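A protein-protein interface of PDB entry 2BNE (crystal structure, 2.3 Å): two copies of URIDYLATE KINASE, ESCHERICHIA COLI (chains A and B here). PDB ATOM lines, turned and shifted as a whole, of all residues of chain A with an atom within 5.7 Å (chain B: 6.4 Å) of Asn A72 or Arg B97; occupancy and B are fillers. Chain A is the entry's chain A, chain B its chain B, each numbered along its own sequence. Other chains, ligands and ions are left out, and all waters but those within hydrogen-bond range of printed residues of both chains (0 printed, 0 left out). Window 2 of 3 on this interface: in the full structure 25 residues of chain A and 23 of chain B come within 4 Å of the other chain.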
ATOM      1  N   ALA A  67     -24.571 -31.526   8.255  1.00  0.00           N
ATOM      2  CA  ALA A  67     -25.330 -31.075   7.097  1.00  0.00           C
ATOM      3  C   ALA A  67     -26.818 -31.386   7.266  1.00  0.00           C
ATOM      4  O   ALA A  67     -27.670 -30.539   7.001  1.00  0.00           O
ATOM      5  CB  ALA A  67     -24.793 -31.733   5.830  1.00  0.00           C
ATOM      6  N   GLY A  70     -28.746 -29.031   8.910  1.00  0.00           N
ATOM      7  CA  GLY A  70     -28.941 -27.765   8.212  1.00  0.00           C
ATOM      8  C   GLY A  70     -27.703 -26.995   7.772  1.00  0.00           C
ATOM      9  O   GLY A  70     -27.778 -26.096   6.931  1.00  0.00           O
ATOM     10  N   MET A  71     -26.553 -27.348   8.327  1.00  0.00           N
ATOM     11  CA  MET A  71     -25.309 -26.661   7.997  1.00  0.00           C
ATOM     12  C   MET A  71     -24.820 -26.946   6.579  1.00  0.00           C
ATOM     13  O   MET A  71     -25.110 -28.000   6.013  1.00  0.00           O
ATOM     14  CB  MET A  71     -24.237 -27.073   8.997  1.00  0.00           C
ATOM     15  CG  MET A  71     -22.955 -26.300   8.905  1.00  0.00           C
ATOM     16  SD  MET A  71     -21.768 -26.930  10.096  1.00  0.00           S
ATOM     17  CE  MET A  71     -22.495 -26.387  11.609  1.00  0.00           C
ATOM     18  N   ASN A  72     -24.087 -26.002   5.998  1.00  0.00           N
ATOM     19  CA  ASN A  72     -23.542 -26.218   4.663  1.00  0.00           C
ATOM     20  C   ASN A  72     -22.571 -27.388   4.792  1.00  0.00           C
ATOM     21  O   ASN A  72     -21.719 -27.404   5.684  1.00  0.00           O
ATOM     22  CB  ASN A  72     -22.799 -24.974   4.162  1.00  0.00           C
ATOM     23  CG  ASN A  72     -23.743 -23.863   3.735  1.00  0.00           C
ATOM     24  OD1 ASN A  72     -24.654 -24.086   2.931  1.00  0.00           O
ATOM     25  ND2 ASN A  72     -23.527 -22.655   4.264  1.00  0.00           N
ATOM     26  N   ARG A  73     -22.707 -28.367   3.910  1.00  0.00           N
ATOM     27  CA  ARG A  73     -21.858 -29.544   3.957  1.00  0.00           C
ATOM     28  C   ARG A  73     -20.356 -29.231   3.983  1.00  0.00           C
ATOM     29  O   ARG A  73     -19.600 -29.866   4.727  1.00  0.00           O
ATOM     30  CB  ARG A  73     -22.191 -30.475   2.777  1.00  0.00           C
ATOM     31  CG  ARG A  73     -21.354 -31.739   2.706  1.00  0.00           C
ATOM     32  CD  ARG A  73     -21.361 -32.510   4.021  1.00  0.00           C
ATOM     33  NE  ARG A  73     -20.454 -33.653   3.962  1.00  0.00           N
ATOM     34  CZ  ARG A  73     -20.709 -34.785   3.308  1.00  0.00           C
ATOM     35  NH1 ARG A  73     -21.858 -34.941   2.663  1.00  0.00           N
ATOM     36  NH2 ARG A  73     -19.796 -35.751   3.272  1.00  0.00           N
ATOM     37  N   VAL A  74     -19.917 -28.265   3.188  1.00  0.00           N
ATOM     38  CA  VAL A  74     -18.489 -27.941   3.171  1.00  0.00           C
ATOM     39  C   VAL A  74     -17.993 -27.470   4.533  1.00  0.00           C
ATOM     40  O   VAL A  74     -16.935 -27.900   4.993  1.00  0.00           O
ATOM     41  CB  VAL A  74     -18.145 -26.879   2.096  1.00  0.00           C
ATOM     42  CG1 VAL A  74     -16.689 -26.474   2.205  1.00  0.00           C
ATOM     43  CG2 VAL A  74     -18.406 -27.450   0.705  1.00  0.00           C
ATOM     44  N   VAL A  75     -18.755 -26.602   5.185  1.00  0.00           N
ATOM     45  CA  VAL A  75     -18.367 -26.119   6.503  1.00  0.00           C
ATOM     46  C   VAL A  75     -18.430 -27.268   7.513  1.00  0.00           C
ATOM     47  O   VAL A  75     -17.633 -27.332   8.453  1.00  0.00           O
ATOM     48  CB  VAL A  75     -19.284 -24.970   6.983  1.00  0.00           C
ATOM     49  CG1 VAL A  75     -18.830 -24.492   8.344  1.00  0.00           C
ATOM     50  CG2 VAL A  75     -19.251 -23.827   5.973  1.00  0.00           C
ATOM     51  N   GLY A  76     -19.386 -28.168   7.315  1.00  0.00           N
ATOM     52  CA  GLY A  76     -19.507 -29.306   8.202  1.00  0.00           C
ATOM     53  C   GLY A  76     -18.274 -30.182   8.079  1.00  0.00           C
ATOM     54  O   GLY A  76     -17.756 -30.686   9.084  1.00  0.00           O
ATOM     55  N   ASP A  77     -17.804 -30.371   6.848  1.00  0.00           N
ATOM     56  CA  ASP A  77     -16.621 -31.183   6.612  1.00  0.00           C
ATOM     57  C   ASP A  77     -15.362 -30.489   7.139  1.00  0.00           C
ATOM     58  O   ASP A  77     -14.419 -31.153   7.584  1.00  0.00           O
ATOM     59  CB  ASP A  77     -16.463 -31.507   5.118  1.00  0.00           C
ATOM     60  CG  ASP A  77     -17.399 -32.621   4.653  1.00  0.00           C
ATOM     61  OD1 ASP A  77     -17.900 -33.391   5.498  1.00  0.00           O
ATOM     62  OD2 ASP A  77     -17.632 -32.740   3.431  1.00  0.00           O
ATOM     63  N   ALA B  31     -27.796 -26.902  16.852  1.00  0.00           N
ATOM     64  CA  ALA B  31     -28.133 -26.180  15.629  1.00  0.00           C
ATOM     65  C   ALA B  31     -29.196 -25.094  15.809  1.00  0.00           C
ATOM     66  O   ALA B  31     -29.036 -23.979  15.308  1.00  0.00           O
ATOM     67  CB  ALA B  31     -28.586 -27.169  14.553  1.00  0.00           C
ATOM     68  N   LEU B  34     -27.872 -21.905  17.398  1.00  0.00           N
ATOM     69  CA  LEU B  34     -27.036 -21.180  16.454  1.00  0.00           C
ATOM     70  C   LEU B  34     -27.923 -20.433  15.465  1.00  0.00           C
ATOM     71  O   LEU B  34     -27.671 -19.272  15.127  1.00  0.00           O
ATOM     72  CB  LEU B  34     -26.160 -22.166  15.692  1.00  0.00           C
ATOM     73  CG  LEU B  34     -24.643 -22.138  15.849  1.00  0.00           C
ATOM     74  CD1 LEU B  34     -24.233 -21.926  17.296  1.00  0.00           C
ATOM     75  CD2 LEU B  34     -24.113 -23.455  15.318  1.00  0.00           C
ATOM     76  N   ASP B  35     -28.962 -21.117  14.998  1.00  0.00           N
ATOM     77  CA  ASP B  35     -29.892 -20.530  14.048  1.00  0.00           C
ATOM     78  C   ASP B  35     -30.631 -19.345  14.639  1.00  0.00           C
ATOM     79  O   ASP B  35     -30.913 -18.384  13.941  1.00  0.00           O
ATOM     80  CB  ASP B  35     -30.885 -21.590  13.567  1.00  0.00           C
ATOM     81  CG  ASP B  35     -30.338 -22.415  12.410  1.00  0.00           C
ATOM     82  OD1 ASP B  35     -30.951 -23.448  12.075  1.00  0.00           O
ATOM     83  OD2 ASP B  35     -29.301 -22.015  11.828  1.00  0.00           O
ATOM     84  N   GLN B  39     -30.301 -15.047  13.782  1.00  0.00           N
ATOM     85  CA  GLN B  39     -31.428 -14.152  13.578  1.00  0.00           C
ATOM     86  C   GLN B  39     -31.321 -12.916  14.475  1.00  0.00           C
ATOM     87  O   GLN B  39     -31.641 -11.804  14.053  1.00  0.00           O
ATOM     88  CB  GLN B  39     -32.743 -14.884  13.871  1.00  0.00           C
ATOM     89  CG  GLN B  39     -33.157 -15.905  12.814  1.00  0.00           C
ATOM     90  CD  GLN B  39     -33.367 -15.282  11.431  1.00  0.00           C
ATOM     91  OE1 GLN B  39     -34.070 -14.278  11.286  1.00  0.00           O
ATOM     92  NE2 GLN B  39     -32.769 -15.884  10.416  1.00  0.00           N
ATOM     93  N   ALA B  90     -19.193 -22.942  12.868  1.00  0.00           N
ATOM     94  CA  ALA B  90     -20.623 -23.218  12.886  1.00  0.00           C
ATOM     95  C   ALA B  90     -21.424 -21.918  12.970  1.00  0.00           C
ATOM     96  O   ALA B  90     -22.420 -21.760  12.290  1.00  0.00           O
ATOM     97  CB  ALA B  90     -20.967 -24.127  14.061  1.00  0.00           C
ATOM     98  N   ARG B  92     -20.477 -18.845  12.022  1.00  0.00           N
ATOM     99  CA  ARG B  92     -20.373 -18.109  10.772  1.00  0.00           C
ATOM    100  C   ARG B  92     -21.356 -18.688   9.773  1.00  0.00           C
ATOM    101  O   ARG B  92     -22.115 -17.951   9.138  1.00  0.00           O
ATOM    102  CB  ARG B  92     -18.968 -18.195  10.180  1.00  0.00           C
ATOM    103  CG  ARG B  92     -18.791 -17.312   8.941  1.00  0.00           C
ATOM    104  CD  ARG B  92     -17.553 -17.696   8.140  1.00  0.00           C
ATOM    105  NE  ARG B  92     -17.698 -19.015   7.546  1.00  0.00           N
ATOM    106  CZ  ARG B  92     -16.689 -19.750   7.085  1.00  0.00           C
ATOM    107  NH1 ARG B  92     -15.445 -19.300   7.147  1.00  0.00           N
ATOM    108  NH2 ARG B  92     -16.931 -20.940   6.558  1.00  0.00           N
ATOM    109  N   ASP B  93     -21.356 -20.008   9.638  1.00  0.00           N
ATOM    110  CA  ASP B  93     -22.266 -20.632   8.700  1.00  0.00           C
ATOM    111  C   ASP B  93     -23.721 -20.286   8.987  1.00  0.00           C
ATOM    112  O   ASP B  93     -24.488 -20.019   8.065  1.00  0.00           O
ATOM    113  CB  ASP B  93     -22.110 -22.150   8.692  1.00  0.00           C
ATOM    114  CG  ASP B  93     -22.713 -22.767   7.455  1.00  0.00           C
ATOM    115  OD1 ASP B  93     -22.276 -22.394   6.339  1.00  0.00           O
ATOM    116  OD2 ASP B  93     -23.621 -23.601   7.586  1.00  0.00           O
ATOM    117  N   ALA B  94     -24.105 -20.309  10.262  1.00  0.00           N
ATOM    118  CA  ALA B  94     -25.472 -19.971  10.639  1.00  0.00           C
ATOM    119  C   ALA B  94     -25.759 -18.533  10.181  1.00  0.00           C
ATOM    120  O   ALA B  94     -26.866 -18.210   9.754  1.00  0.00           O
ATOM    121  CB  ALA B  94     -25.642 -20.089  12.146  1.00  0.00           C
ATOM    122  N   LEU B  95     -24.747 -17.678  10.272  1.00  0.00           N
ATOM    123  CA  LEU B  95     -24.877 -16.285   9.854  1.00  0.00           C
ATOM    124  C   LEU B  95     -25.038 -16.211   8.331  1.00  0.00           C
ATOM    125  O   LEU B  95     -25.893 -15.491   7.818  1.00  0.00           O
ATOM    126  CB  LEU B  95     -23.642 -15.491  10.297  1.00  0.00           C
ATOM    127  CG  LEU B  95     -23.695 -14.532  11.503  1.00  0.00           C
ATOM    128  CD1 LEU B  95     -24.995 -14.651  12.255  1.00  0.00           C
ATOM    129  CD2 LEU B  95     -22.506 -14.794  12.412  1.00  0.00           C
ATOM    130  N   HIS B  96     -24.230 -16.964   7.599  1.00  0.00           N
ATOM    131  CA  HIS B  96     -24.337 -16.936   6.142  1.00  0.00           C
ATOM    132  C   HIS B  96     -25.679 -17.466   5.670  1.00  0.00           C
ATOM    133  O   HIS B  96     -26.297 -16.881   4.782  1.00  0.00           O
ATOM    134  CB  HIS B  96     -23.212 -17.745   5.510  1.00  0.00           C
ATOM    135  CG  HIS B  96     -21.872 -17.086   5.616  1.00  0.00           C
ATOM    136  ND1 HIS B  96     -20.704 -17.709   5.237  1.00  0.00           N
ATOM    137  CD2 HIS B  96     -21.519 -15.851   6.047  1.00  0.00           C
ATOM    138  CE1 HIS B  96     -19.688 -16.887   5.427  1.00  0.00           C
ATOM    139  NE2 HIS B  96     -20.155 -15.752   5.917  1.00  0.00           N
ATOM    140  N   ARG B  97     -26.144 -18.559   6.271  1.00  0.00           N
ATOM    141  CA  ARG B  97     -27.424 -19.124   5.861  1.00  0.00           C
ATOM    142  C   ARG B  97     -28.581 -18.211   6.226  1.00  0.00           C
ATOM    143  O   ARG B  97     -29.685 -18.373   5.720  1.00  0.00           O
ATOM    144  CB  ARG B  97     -27.617 -20.529   6.447  1.00  0.00           C
ATOM    145  CG  ARG B  97     -26.738 -21.563   5.759  1.00  0.00           C
ATOM    146  CD  ARG B  97     -26.893 -22.984   6.305  1.00  0.00           C
ATOM    147  NE  ARG B  97     -26.434 -23.138   7.681  1.00  0.00           N
ATOM    148  CZ  ARG B  97     -27.214 -23.056   8.756  1.00  0.00           C
ATOM    149  NH1 ARG B  97     -28.512 -22.817   8.633  1.00  0.00           N
ATOM    150  NH2 ARG B  97     -26.697 -23.219   9.965  1.00  0.00           N
ATOM    151  N   ALA B  98     -28.321 -17.245   7.100  1.00  0.00           N
ATOM    152  CA  ALA B  98     -29.342 -16.281   7.501  1.00  0.00           C
ATOM    153  C   ALA B  98     -29.142 -15.000   6.680  1.00  0.00           C
ATOM    154  O   ALA B  98     -29.751 -13.963   6.944  1.00  0.00           O
ATOM    155  CB  ALA B  98     -29.228 -15.980   8.991  1.00  0.00           C
ATOM    156  N   TYR B  99     -28.261 -15.084   5.689  1.00  0.00           N
ATOM    157  CA  TYR B  99     -27.967 -13.967   4.811  1.00  0.00           C
ATOM    158  C   TYR B  99     -27.388 -12.776   5.550  1.00  0.00           C
ATOM    159  O   TYR B  99     -27.794 -11.626   5.354  1.00  0.00           O
ATOM    160  CB  TYR B  99     -29.231 -13.593   4.039  1.00  0.00           C
ATOM    161  CG  TYR B  99     -29.743 -14.774   3.252  1.00  0.00           C
ATOM    162  CD1 TYR B  99     -29.083 -15.204   2.099  1.00  0.00           C
ATOM    163  CD2 TYR B  99     -30.822 -15.529   3.716  1.00  0.00           C
ATOM    164  CE1 TYR B  99     -29.480 -16.358   1.434  1.00  0.00           C
ATOM    165  CE2 TYR B  99     -31.228 -16.691   3.055  1.00  0.00           C
ATOM    166  CZ  TYR B  99     -30.551 -17.098   1.918  1.00  0.00           C
ATOM    167  OH  TYR B  99     -30.935 -18.254   1.269  1.00  0.00           O
ATOM    168  N   VAL B 100     -26.429 -13.070   6.416  1.00  0.00           N
ATOM    169  CA  VAL B 100     -25.749 -12.032   7.162  1.00  0.00           C
ATOM    170  C   VAL B 100     -24.287 -12.082   6.741  1.00  0.00           C
ATOM    171  O   VAL B 100     -23.667 -13.139   6.766  1.00  0.00           O
ATOM    172  CB  VAL B 100     -25.881 -12.271   8.679  1.00  0.00           C
ATOM    173  CG1 VAL B 100     -25.088 -11.214   9.455  1.00  0.00           C
ATOM    174  CG2 VAL B 100     -27.341 -12.224   9.067  1.00  0.00           C
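Asn A72 touches just these residues of chain B: Asp B93 and Arg B97.
Of chain A, only Gly A70 (3.3 Å), Met A71 (3.7 Å) and Asn A72 (3.7 Å) come within 4 Å of Arg B97.
Of the printed residues of chain A, Ala B90 touches Met A71 (3.7 Å).
Printed residues of chain B within 4 Å of Val A75: Arg B92 (3.7 Å) and Asp B93 (3.4 Å).
Of the printed residues of chain B, Met A71 touches Ala B90 (3.7 Å), Asp B93 (3.1 Å) and Arg B97 (3.7 Å).
Val A74 touches none of the printed residues of chain B.
The nearest residue of chain B that does not touch Asn A72 is His B96 (5.1 Å).
The guanidinium group (NE) of Arg B97 lies within salt-bridge range of the side-chain carboxylate (OD2) of Asp B93 (2.9 Å).
The side-chain carboxylate of Asp B35 lies within salt-bridge range of the guanidinium group of Arg B97 (3.4 Å).
ND2 of Asn A72 is in hydrogen-bond range of OD1 of Asp B93.
The backbone carbonyl oxygen of Gly A70 sits close to the guanidinium group of Arg B97, at 3.3 Å.
Among the printed residues, merely in contact across the chains: Met A71 with Ala B90, Met A71 with Asp B93, Met A71 with Arg B97, Asn A72 with Arg B97, Val A75 with Arg B92 and Val A75 with Asp B93.
No position is printed for both chains.
Of the 9 printed residues of chain A, 4 touch a printed residue of chain B.
Hydrophobic or aromatic side chains of chain A that line the printed part of chain B: Met A71 and Val A75.
Among the printed residues, 8 pairs touch across the chains.
Among the printed residues, no Asp or Glu carboxylate lies within 4 Å of a Lys or Arg side-chain nitrogen of the other chain.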
